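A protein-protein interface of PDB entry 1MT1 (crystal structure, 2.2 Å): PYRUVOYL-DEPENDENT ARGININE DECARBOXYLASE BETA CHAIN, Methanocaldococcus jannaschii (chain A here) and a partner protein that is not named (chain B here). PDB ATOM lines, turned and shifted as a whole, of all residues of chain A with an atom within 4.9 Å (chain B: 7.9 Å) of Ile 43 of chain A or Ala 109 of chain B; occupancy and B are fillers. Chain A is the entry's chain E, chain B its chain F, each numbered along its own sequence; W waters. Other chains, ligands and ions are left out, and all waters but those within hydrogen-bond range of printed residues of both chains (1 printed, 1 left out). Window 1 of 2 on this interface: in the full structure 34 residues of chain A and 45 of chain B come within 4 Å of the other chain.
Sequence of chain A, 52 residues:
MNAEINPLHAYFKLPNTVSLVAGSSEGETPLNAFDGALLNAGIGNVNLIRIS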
ATOM      1  N   THR A  17      20.254  -0.329 -13.179  1.00  0.00           N
ATOM      2  CA  THR A  17      19.099  -1.194 -13.247  1.00  0.00           C
ATOM      3  C   THR A  17      18.212  -0.834 -14.449  1.00  0.00           C
ATOM      4  O   THR A  17      18.182   0.318 -14.884  1.00  0.00           O
ATOM      5  CB  THR A  17      18.320  -1.060 -11.902  1.00  0.00           C
ATOM      6  OG1 THR A  17      18.725  -2.099 -11.000  1.00  0.00           O
ATOM      7  CG2 THR A  17      16.846  -1.092 -12.094  1.00  0.00           C
ATOM      8  N   VAL A  18      17.527  -1.831 -15.006  1.00  0.00           N
ATOM      9  CA  VAL A  18      16.622  -1.624 -16.136  1.00  0.00           C
ATOM     10  C   VAL A  18      15.395  -2.529 -15.978  1.00  0.00           C
ATOM     11  O   VAL A  18      15.522  -3.718 -15.685  1.00  0.00           O
ATOM     12  CB  VAL A  18      17.323  -1.858 -17.511  1.00  0.00           C
ATOM     13  CG1 VAL A  18      18.003  -3.215 -17.549  1.00  0.00           C
ATOM     14  CG2 VAL A  18      16.315  -1.735 -18.651  1.00  0.00           C
ATOM     15  N   SER A  19      14.209  -1.950 -16.155  1.00  0.00           N
ATOM     16  CA  SER A  19      12.958  -2.677 -16.003  1.00  0.00           C
ATOM     17  C   SER A  19      12.078  -2.509 -17.227  1.00  0.00           C
ATOM     18  O   SER A  19      11.912  -1.400 -17.728  1.00  0.00           O
ATOM     19  CB  SER A  19      12.191  -2.174 -14.779  1.00  0.00           C
ATOM     20  OG  SER A  19      12.969  -2.263 -13.596  1.00  0.00           O
ATOM     21  N   VAL A  21       8.456  -2.587 -18.856  1.00  0.00           N
ATOM     22  CA  VAL A  21       7.051  -2.454 -18.496  1.00  0.00           C
ATOM     23  C   VAL A  21       6.267  -2.185 -19.770  1.00  0.00           C
ATOM     24  O   VAL A  21       6.837  -1.812 -20.795  1.00  0.00           O
ATOM     25  CB  VAL A  21       6.785  -1.314 -17.467  1.00  0.00           C
ATOM     26  CG1 VAL A  21       7.444  -1.639 -16.131  1.00  0.00           C
ATOM     27  CG2 VAL A  21       7.264   0.037 -18.003  1.00  0.00           C
ATOM     28  N   LEU A  38       0.342   4.571 -18.888  1.00  0.00           N
ATOM     29  CA  LEU A  38       1.491   4.614 -17.976  1.00  0.00           C
ATOM     30  C   LEU A  38       1.085   4.023 -16.623  1.00  0.00           C
ATOM     31  O   LEU A  38       1.853   3.280 -16.008  1.00  0.00           O
ATOM     32  CB  LEU A  38       1.999   6.051 -17.778  1.00  0.00           C
ATOM     33  CG  LEU A  38       2.474   6.857 -18.994  1.00  0.00           C
ATOM     34  CD1 LEU A  38       3.037   8.196 -18.540  1.00  0.00           C
ATOM     35  CD2 LEU A  38       3.526   6.106 -19.760  1.00  0.00           C
ATOM     36  N   LEU A  39      -0.115   4.370 -16.159  1.00  0.00           N
ATOM     37  CA  LEU A  39      -0.632   3.855 -14.890  1.00  0.00           C
ATOM     38  C   LEU A  39      -0.833   2.346 -14.983  1.00  0.00           C
ATOM     39  O   LEU A  39      -0.483   1.606 -14.063  1.00  0.00           O
ATOM     40  CB  LEU A  39      -1.963   4.526 -14.539  1.00  0.00           C
ATOM     41  CG  LEU A  39      -1.894   6.002 -14.150  1.00  0.00           C
ATOM     42  CD1 LEU A  39      -3.261   6.669 -14.331  1.00  0.00           C
ATOM     43  CD2 LEU A  39      -1.389   6.132 -12.718  1.00  0.00           C
ATOM     44  N   ALA A  41       0.747   0.473 -16.760  1.00  0.00           N
ATOM     45  CA  ALA A  41       2.096  -0.075 -16.815  1.00  0.00           C
ATOM     46  C   ALA A  41       2.774  -0.038 -15.439  1.00  0.00           C
ATOM     47  O   ALA A  41       3.782  -0.703 -15.218  1.00  0.00           O
ATOM     48  CB  ALA A  41       2.924   0.698 -17.830  1.00  0.00           C
ATOM     49  N   GLY A  42       2.222   0.742 -14.516  1.00  0.00           N
ATOM     50  CA  GLY A  42       2.805   0.826 -13.186  1.00  0.00           C
ATOM     51  C   GLY A  42       3.828   1.934 -13.026  1.00  0.00           C
ATOM     52  O   GLY A  42       4.503   2.013 -12.001  1.00  0.00           O
ATOM     53  N   ILE A  43       3.916   2.795 -14.032  1.00  0.00           N
ATOM     54  CA  ILE A  43       4.868   3.889 -14.030  1.00  0.00           C
ATOM     55  C   ILE A  43       4.126   5.207 -14.307  1.00  0.00           C
ATOM     56  O   ILE A  43       4.670   6.135 -14.907  1.00  0.00           O
ATOM     57  CB  ILE A  43       5.978   3.590 -15.086  1.00  0.00           C
ATOM     58  CG1 ILE A  43       7.218   4.441 -14.839  1.00  0.00           C
ATOM     59  CG2 ILE A  43       5.441   3.753 -16.508  1.00  0.00           C
ATOM     60  CD1 ILE A  43       8.402   4.029 -15.685  1.00  0.00           C
ATOM     61  N   GLY A  44       2.889   5.290 -13.818  1.00  0.00           N
ATOM     62  CA  GLY A  44       2.069   6.476 -14.031  1.00  0.00           C
ATOM     63  C   GLY A  44       2.251   7.733 -13.201  1.00  0.00           C
ATOM     64  O   GLY A  44       1.730   8.794 -13.565  1.00  0.00           O
ATOM     65  N   ASN A  45       2.970   7.645 -12.091  1.00  0.00           N
ATOM     66  CA  ASN A  45       3.150   8.824 -11.258  1.00  0.00           C
ATOM     67  C   ASN A  45       4.590   9.325 -11.174  1.00  0.00           C
ATOM     68  O   ASN A  45       4.997   9.915 -10.176  1.00  0.00           O
ATOM     69  CB  ASN A  45       2.543   8.587  -9.872  1.00  0.00           C
ATOM     70  CG  ASN A  45       1.022   8.411  -9.922  1.00  0.00           C
ATOM     71  OD1 ASN A  45       0.470   7.456  -9.355  1.00  0.00           O
ATOM     72  ND2 ASN A  45       0.339   9.332 -10.607  1.00  0.00           N
ATOM     73  N   VAL A  46       5.346   9.112 -12.250  1.00  0.00           N
ATOM     74  CA  VAL A  46       6.733   9.559 -12.312  1.00  0.00           C
ATOM     75  C   VAL A  46       6.946  10.409 -13.565  1.00  0.00           C
ATOM     76  O   VAL A  46       6.109  10.435 -14.463  1.00  0.00           O
ATOM     77  CB  VAL A  46       7.728   8.368 -12.352  1.00  0.00           C
ATOM     78  CG1 VAL A  46       7.530   7.468 -11.144  1.00  0.00           C
ATOM     79  CG2 VAL A  46       7.569   7.589 -13.635  1.00  0.00           C
ATOM     80  N   LEU A  48       8.875  10.808 -16.820  1.00  0.00           N
ATOM     81  CA  LEU A  48       9.699  10.078 -17.771  1.00  0.00           C
ATOM     82  C   LEU A  48      10.575  11.007 -18.600  1.00  0.00           C
ATOM     83  O   LEU A  48      10.072  11.913 -19.263  1.00  0.00           O
ATOM     84  CB  LEU A  48       8.837   9.250 -18.727  1.00  0.00           C
ATOM     85  CG  LEU A  48       7.881   8.185 -18.195  1.00  0.00           C
ATOM     86  CD1 LEU A  48       7.413   7.347 -19.371  1.00  0.00           C
ATOM     87  CD2 LEU A  48       8.572   7.306 -17.191  1.00  0.00           C
ATOM     88  N   GLU B   8      21.509  -4.610 -14.187  1.00  0.00           N
ATOM     89  CA  GLU B   8      20.721  -5.825 -14.076  1.00  0.00           C
ATOM     90  C   GLU B   8      19.262  -5.604 -14.454  1.00  0.00           C
ATOM     91  O   GLU B   8      18.702  -4.540 -14.189  1.00  0.00           O
ATOM     92  CB  GLU B   8      20.800  -6.346 -12.633  1.00  0.00           C
ATOM     93  CG  GLU B   8      20.139  -7.695 -12.406  1.00  0.00           C
ATOM     94  CD  GLU B   8      19.908  -8.007 -10.936  1.00  0.00           C
ATOM     95  OE1 GLU B   8      20.612  -7.442 -10.074  1.00  0.00           O
ATOM     96  OE2 GLU B   8      19.002  -8.816 -10.638  1.00  0.00           O
ATOM     97  N   VAL B  10      15.627  -6.070 -13.704  1.00  0.00           N
ATOM     98  CA  VAL B  10      14.851  -6.367 -12.503  1.00  0.00           C
ATOM     99  C   VAL B  10      13.407  -5.924 -12.694  1.00  0.00           C
ATOM    100  O   VAL B  10      13.116  -5.086 -13.553  1.00  0.00           O
ATOM    101  CB  VAL B  10      15.400  -5.617 -11.254  1.00  0.00           C
ATOM    102  CG1 VAL B  10      16.858  -5.985 -10.992  1.00  0.00           C
ATOM    103  CG2 VAL B  10      15.238  -4.108 -11.421  1.00  0.00           C
ATOM    104  N   LEU B  12      10.168  -3.839 -12.155  1.00  0.00           N
ATOM    105  CA  LEU B  12      10.062  -2.439 -11.748  1.00  0.00           C
ATOM    106  C   LEU B  12       9.942  -2.249 -10.236  1.00  0.00           C
ATOM    107  O   LEU B  12       9.010  -2.756  -9.613  1.00  0.00           O
ATOM    108  CB  LEU B  12       8.876  -1.765 -12.435  1.00  0.00           C
ATOM    109  CG  LEU B  12       8.811  -0.255 -12.193  1.00  0.00           C
ATOM    110  CD1 LEU B  12       9.851   0.446 -13.055  1.00  0.00           C
ATOM    111  CD2 LEU B  12       7.413   0.252 -12.506  1.00  0.00           C
ATOM    112  N   PRO B  13      10.884  -1.503  -9.633  1.00  0.00           N
ATOM    113  CA  PRO B  13      10.901  -1.231  -8.191  1.00  0.00           C
ATOM    114  C   PRO B  13       9.831  -0.196  -7.841  1.00  0.00           C
ATOM    115  O   PRO B  13       9.135   0.319  -8.725  1.00  0.00           O
ATOM    116  CB  PRO B  13      12.291  -0.614  -7.966  1.00  0.00           C
ATOM    117  CG  PRO B  13      13.046  -0.860  -9.256  1.00  0.00           C
ATOM    118  CD  PRO B  13      11.990  -0.800 -10.300  1.00  0.00           C
ATOM    119  N   LEU B  15       8.865   3.243  -7.243  1.00  0.00           N
ATOM    120  CA  LEU B  15       9.463   4.532  -7.586  1.00  0.00           C
ATOM    121  C   LEU B  15       8.810   5.674  -6.823  1.00  0.00           C
ATOM    122  O   LEU B  15       7.592   5.708  -6.673  1.00  0.00           O
ATOM    123  CB  LEU B  15       9.337   4.790  -9.091  1.00  0.00           C
ATOM    124  CG  LEU B  15       9.872   3.721 -10.043  1.00  0.00           C
ATOM    125  CD1 LEU B  15       9.477   4.040 -11.467  1.00  0.00           C
ATOM    126  CD2 LEU B  15      11.367   3.628  -9.920  1.00  0.00           C
ATOM    127  N   ALA B  19       9.444  11.121  -9.496  1.00  0.00           N
ATOM    128  CA  ALA B  19      10.828  10.787  -9.844  1.00  0.00           C
ATOM    129  C   ALA B  19      11.169  11.050 -11.313  1.00  0.00           C
ATOM    130  O   ALA B  19      10.330  10.861 -12.194  1.00  0.00           O
ATOM    131  CB  ALA B  19      11.110   9.319  -9.508  1.00  0.00           C
ATOM    132  N   VAL B  21      12.797   9.686 -14.178  1.00  0.00           N
ATOM    133  CA  VAL B  21      13.225   8.367 -14.644  1.00  0.00           C
ATOM    134  C   VAL B  21      13.641   8.303 -16.121  1.00  0.00           C
ATOM    135  O   VAL B  21      12.820   8.521 -17.013  1.00  0.00           O
ATOM    136  CB  VAL B  21      12.079   7.340 -14.407  1.00  0.00           C
ATOM    137  CG1 VAL B  21      12.496   5.939 -14.832  1.00  0.00           C
ATOM    138  CG2 VAL B  21      11.637   7.363 -12.937  1.00  0.00           C
ATOM    139  N   PRO B  22      14.930   8.020 -16.395  1.00  0.00           N
ATOM    140  CA  PRO B  22      15.437   7.921 -17.773  1.00  0.00           C
ATOM    141  C   PRO B  22      14.727   6.693 -18.335  1.00  0.00           C
ATOM    142  O   PRO B  22      14.823   5.604 -17.759  1.00  0.00           O
ATOM    143  CB  PRO B  22      16.922   7.642 -17.569  1.00  0.00           C
ATOM    144  CG  PRO B  22      17.216   8.283 -16.246  1.00  0.00           C
ATOM    145  CD  PRO B  22      16.027   7.847 -15.431  1.00  0.00           C
ATOM    146  N   THR B  23      14.010   6.875 -19.440  1.00  0.00           N
ATOM    147  CA  THR B  23      13.231   5.794 -20.030  1.00  0.00           C
ATOM    148  C   THR B  23      13.241   5.773 -21.556  1.00  0.00           C
ATOM    149  O   THR B  23      13.169   6.816 -22.202  1.00  0.00           O
ATOM    150  CB  THR B  23      11.749   5.924 -19.598  1.00  0.00           C
ATOM    151  OG1 THR B  23      11.679   6.220 -18.198  1.00  0.00           O
ATOM    152  CG2 THR B  23      10.979   4.648 -19.881  1.00  0.00           C
ATOM    153  N   ALA B  24      13.333   4.569 -22.118  1.00  0.00           N
ATOM    154  CA  ALA B  24      13.294   4.376 -23.559  1.00  0.00           C
ATOM    155  C   ALA B  24      11.889   3.812 -23.717  1.00  0.00           C
ATOM    156  O   ALA B  24      11.493   2.925 -22.955  1.00  0.00           O
ATOM    157  CB  ALA B  24      14.315   3.337 -24.002  1.00  0.00           C
ATOM    158  N   TYR B  25      11.108   4.349 -24.646  1.00  0.00           N
ATOM    159  CA  TYR B  25       9.769   3.832 -24.824  1.00  0.00           C
ATOM    160  C   TYR B  25       9.152   4.011 -26.193  1.00  0.00           C
ATOM    161  O   TYR B  25       9.606   4.803 -27.020  1.00  0.00           O
ATOM    162  CB  TYR B  25       8.816   4.384 -23.754  1.00  0.00           C
ATOM    163  CG  TYR B  25       8.580   5.876 -23.796  1.00  0.00           C
ATOM    164  CD1 TYR B  25       7.646   6.434 -24.667  1.00  0.00           C
ATOM    165  CD2 TYR B  25       9.250   6.725 -22.926  1.00  0.00           C
ATOM    166  CE1 TYR B  25       7.386   7.806 -24.662  1.00  0.00           C
ATOM    167  CE2 TYR B  25       8.998   8.087 -22.911  1.00  0.00           C
ATOM    168  CZ  TYR B  25       8.069   8.620 -23.777  1.00  0.00           C
ATOM    169  OH  TYR B  25       7.826   9.975 -23.751  1.00  0.00           O
ATOM    170  N   ILE B  41       9.143  -3.521 -26.554  1.00  0.00           N
ATOM    171  CA  ILE B  41      10.462  -3.073 -26.126  1.00  0.00           C
ATOM    172  C   ILE B  41      11.365  -4.287 -25.985  1.00  0.00           C
ATOM    173  O   ILE B  41      10.917  -5.344 -25.545  1.00  0.00           O
ATOM    174  CB  ILE B  41      10.386  -2.347 -24.736  1.00  0.00           C
ATOM    175  CG1 ILE B  41      10.047  -0.872 -24.915  1.00  0.00           C
ATOM    176  CG2 ILE B  41      11.716  -2.451 -23.992  1.00  0.00           C
ATOM    177  CD1 ILE B  41      11.256   0.014 -25.185  1.00  0.00           C
ATOM    178  N   VAL B  43      15.638  -5.520 -25.020  1.00  0.00           N
ATOM    179  CA  VAL B  43      16.941  -5.154 -24.478  1.00  0.00           C
ATOM    180  C   VAL B  43      17.908  -6.285 -24.813  1.00  0.00           C
ATOM    181  O   VAL B  43      17.745  -7.410 -24.336  1.00  0.00           O
ATOM    182  CB  VAL B  43      16.926  -4.988 -22.937  1.00  0.00           C
ATOM    183  CG1 VAL B  43      18.305  -4.542 -22.455  1.00  0.00           C
ATOM    184  CG2 VAL B  43      15.870  -3.983 -22.515  1.00  0.00           C
ATOM    185  N   ILE B  55      18.834  -1.056 -26.156  1.00  0.00           N
ATOM    186  CA  ILE B  55      17.387  -1.019 -25.994  1.00  0.00           C
ATOM    187  C   ILE B  55      16.754  -0.555 -27.302  1.00  0.00           C
ATOM    188  O   ILE B  55      17.171   0.446 -27.880  1.00  0.00           O
ATOM    189  CB  ILE B  55      16.986  -0.036 -24.879  1.00  0.00           C
ATOM    190  CG1 ILE B  55      17.710  -0.402 -23.575  1.00  0.00           C
ATOM    191  CG2 ILE B  55      15.468  -0.021 -24.705  1.00  0.00           C
ATOM    192  CD1 ILE B  55      17.576   0.652 -22.475  1.00  0.00           C
ATOM    193  N   PHE B 105       1.544   1.172 -24.895  1.00  0.00           N
ATOM    194  CA  PHE B 105       2.831   1.691 -24.445  1.00  0.00           C
ATOM    195  C   PHE B 105       3.748   0.606 -23.868  1.00  0.00           C
ATOM    196  O   PHE B 105       3.308  -0.245 -23.095  1.00  0.00           O
ATOM    197  CB  PHE B 105       2.536   2.787 -23.397  1.00  0.00           C
ATOM    198  CG  PHE B 105       3.725   3.221 -22.571  1.00  0.00           C
ATOM    199  CD1 PHE B 105       4.493   4.314 -22.952  1.00  0.00           C
ATOM    200  CD2 PHE B 105       4.033   2.574 -21.379  1.00  0.00           C
ATOM    201  CE1 PHE B 105       5.551   4.762 -22.157  1.00  0.00           C
ATOM    202  CE2 PHE B 105       5.085   3.012 -20.580  1.00  0.00           C
ATOM    203  CZ  PHE B 105       5.846   4.112 -20.972  1.00  0.00           C
ATOM    204  N   ALA B 106       5.023   0.642 -24.248  1.00  0.00           N
ATOM    205  CA  ALA B 106       6.021  -0.314 -23.746  1.00  0.00           C
ATOM    206  C   ALA B 106       7.280   0.491 -23.448  1.00  0.00           C
ATOM    207  O   ALA B 106       7.662   1.363 -24.234  1.00  0.00           O
ATOM    208  CB  ALA B 106       6.311  -1.398 -24.782  1.00  0.00           C
ATOM    209  N   ALA B 107       7.939   0.191 -22.332  1.00  0.00           N
ATOM    210  CA  ALA B 107       9.127   0.940 -21.950  1.00  0.00           C
ATOM    211  C   ALA B 107      10.163   0.159 -21.183  1.00  0.00           C
ATOM    212  O   ALA B 107       9.878  -0.886 -20.610  1.00  0.00           O
ATOM    213  CB  ALA B 107       8.723   2.150 -21.123  1.00  0.00           C
ATOM    214  N   ALA B 108      11.370   0.719 -21.168  1.00  0.00           N
ATOM    215  CA  ALA B 108      12.497   0.169 -20.435  1.00  0.00           C
ATOM    216  C   ALA B 108      12.915   1.332 -19.547  1.00  0.00           C
ATOM    217  O   ALA B 108      13.414   2.350 -20.032  1.00  0.00           O
ATOM    218  CB  ALA B 108      13.637  -0.223 -21.384  1.00  0.00           C
ATOM    219  N   ALA B 109      12.659   1.199 -18.254  1.00  0.00           N
ATOM    220  CA  ALA B 109      12.976   2.247 -17.294  1.00  0.00           C
ATOM    221  C   ALA B 109      14.311   2.018 -16.600  1.00  0.00           C
ATOM    222  O   ALA B 109      14.505   0.992 -15.949  1.00  0.00           O
ATOM    223  CB  ALA B 109      11.863   2.342 -16.258  1.00  0.00           C
ATOM    224  N   LEU B 110      15.222   2.977 -16.736  1.00  0.00           N
ATOM    225  CA  LEU B 110      16.536   2.886 -16.103  1.00  0.00           C
ATOM    226  C   LEU B 110      16.424   3.437 -14.695  1.00  0.00           C
ATOM    227  O   LEU B 110      15.919   4.546 -14.493  1.00  0.00           O
ATOM    228  CB  LEU B 110      17.582   3.696 -16.875  1.00  0.00           C
ATOM    229  CG  LEU B 110      17.906   3.346 -18.331  1.00  0.00           C
ATOM    230  CD1 LEU B 110      19.111   4.158 -18.805  1.00  0.00           C
ATOM    231  CD2 LEU B 110      18.216   1.885 -18.456  1.00  0.00           C
ATOM    232  N   TRP B 111      16.871   2.662 -13.713  1.00  0.00           N
ATOM    233  CA  TRP B 111      16.794   3.125 -12.334  1.00  0.00           C
ATOM    234  C   TRP B 111      18.031   2.731 -11.530  1.00  0.00           C
ATOM    235  O   TRP B 111      19.062   2.362 -12.101  1.00  0.00           O
ATOM    236  CB  TRP B 111      15.494   2.642 -11.675  1.00  0.00           C
ATOM    237  CG  TRP B 111      15.107   3.416 -10.438  1.00  0.00           C
ATOM    238  CD1 TRP B 111      14.828   2.896  -9.203  1.00  0.00           C
ATOM    239  CD2 TRP B 111      14.992   4.843 -10.305  1.00  0.00           C
ATOM    240  NE1 TRP B 111      14.553   3.911  -8.310  1.00  0.00           N
ATOM    241  CE2 TRP B 111      14.648   5.113  -8.959  1.00  0.00           C
ATOM    242  CE3 TRP B 111      15.149   5.918 -11.190  1.00  0.00           C
ATOM    243  CZ2 TRP B 111      14.458   6.412  -8.478  1.00  0.00           C
ATOM    244  CZ3 TRP B 111      14.961   7.212 -10.712  1.00  0.00           C
ATOM    245  CH2 TRP B 111      14.619   7.447  -9.367  1.00  0.00           C
ATOM    246  N   TYR B 112      17.925   2.814 -10.208  1.00  0.00           N
ATOM    247  CA  TYR B 112      19.041   2.524  -9.320  1.00  0.00           C
ATOM    248  C   TYR B 112      18.738   1.456  -8.279  1.00  0.00           C
ATOM    249  O   TYR B 112      17.612   1.338  -7.797  1.00  0.00           O
ATOM    250  CB  TYR B 112      19.475   3.814  -8.621  1.00  0.00           C
ATOM    251  CG  TYR B 112      19.854   4.915  -9.580  1.00  0.00           C
ATOM    252  CD1 TYR B 112      21.188   5.171  -9.874  1.00  0.00           C
ATOM    253  CD2 TYR B 112      18.882   5.688 -10.210  1.00  0.00           C
ATOM    254  CE1 TYR B 112      21.548   6.164 -10.769  1.00  0.00           C
ATOM    255  CE2 TYR B 112      19.234   6.688 -11.117  1.00  0.00           C
ATOM    256  CZ  TYR B 112      20.574   6.916 -11.390  1.00  0.00           C
ATOM    257  OH  TYR B 112      20.950   7.897 -12.284  1.00  0.00           O
HETATM  258  O   HOH W   1      16.073  -0.464  -9.420  1.00  0.00           O
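N of Ile 43 of chain A sits at hydrogen-bond distance from O of Leu 38 of chain A. N of Gly 44 of chain A lies within hydrogen-bond range of O of Leu 38 of chain A, at 3.1 Å. O of Val 21 of chain B sits at hydrogen-bond distance from OG1 of Thr 23 of chain B, at 2.8 Å. The backbone NH (N) of Leu 110 of chain B sits at hydrogen-bond distance from the backbone carbonyl oxygen (O) of Pro 22 of chain B. The backbone carbonyl oxygen (O) of Ala 24 of chain B is in hydrogen-bond range of the backbone NH (N) of Ala 108 of chain B (2.8 Å).
The backbone carbonyl oxygen of Thr 17 of chain A sits at hydrogen-bond distance from the backbone NH of Trp 111 of chain B, 2.9 Å away. The backbone NH of Val 18 of chain A is in hydrogen-bond range of the backbone carbonyl oxygen of Glu 8 of chain B (3.1 Å). The backbone carbonyl oxygen (O) of Val 18 of chain A lies within hydrogen-bond range of the backbone NH (N) of Val 10 of chain B (3.1 Å). OG of Ser 19 of chain A sits at hydrogen-bond distance from O of Val 10 of chain B, at 2.8 Å. The backbone NH (N) of Ala 109 of chain B is in hydrogen-bond range of the backbone carbonyl oxygen (O) of Ser 19 of chain A. The backbone carbonyl oxygen (O) of Val 21 of chain A lies within hydrogen-bond range of the backbone NH (N) of Ala 107 of chain B.
Of the printed residues of chain B, Thr 17 of chain A touches Glu 8 (3.5 Å), Val 10 (3.5 Å), Ala 109 (3.9 Å), Leu 110 (3.3 Å) and Trp 111 (2.9 Å). Of the printed residues of chain B, Gly 42 of chain A touches Leu 12 (3.4 Å). Asn 45 of chain A touches none of the printed residues of chain B. Of the printed residues of chain A, Val 10 of chain B touches Thr 17, Val 18 and Ser 19. Of the printed residues of chain A, Thr 23 of chain B touches Leu 48 (3.4 Å). Of the printed residues of chain A, Ala 109 of chain B touches Thr 17 (3.9 Å), Val 18 (3.4 Å), Ser 19 (2.8 Å) and Ile 43 (3.9 Å). The nearest printed residue of chain B that does not touch Ile 43 of chain A is Leu 15 of chain B (4.1 Å). The nearest printed residue of chain A that does not touch Val 21 of chain B is Val 46 of chain A (4.1 Å).
Val 10 of chain B touches Thr 17 of chain A. CA of Leu 110 of chain B touches O of Thr 17 of chain A (3.3 Å). Leu 110 of chain B touches Val 18 of chain A (CD2 to CB, 3.96 Å). Ala 107 of chain B touches Ser 19 of chain A. CA of Ala 108 of chain B touches O of Ser 19 of chain A, at 3.2 Å. Leu 38 of chain A touches Phe 105 of chain B. Leu 12 of chain B touches Gly 42 of chain A (CD2 to O, 3.4 Å). CB of Val 46 of chain A touches O of Ala 19 of chain B, at 3.6 Å. OG1 of Thr 23 of chain B touches CD2 of Leu 48 of chain A, at 3.4 Å. Phe 105 of chain B touches Leu 48 of chain A.
Water W1 bridges the backbone carbonyl oxygen (O) of Tyr 112 of chain B and the side-chain hydroxyl (OG1) of Thr 17 of chain A.
Printed residues of chain A that touch a printed residue of chain B: Thr 17, Val 18, Ser 19, Val 21, Leu 38, Gly 42, Ile 43, Val 46 and Leu 48. Printed residues of chain B that touch a printed residue of chain A: Glu 8, Val 10, Leu 12, Pro 13, Leu 15, Ala 19, Val 21, Thr 23, Tyr 25, Phe 105, Ala 106, Ala 107, Ala 108, Ala 109, Leu 110 and Trp 111. Hydrophobic or aromatic side chains of chain B that line the printed part of chain A: Val 10, Leu 12, Pro 13, Leu 15, Tyr 25, Phe 105, Ala 109, Leu 110 and Trp 111. Among the printed residues, 27 pairs touch across the chains. Among the printed residues, no Asp or Glu carboxylate lies within 4 Å of a Lys or Arg side-chain nitrogen of the other chain.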
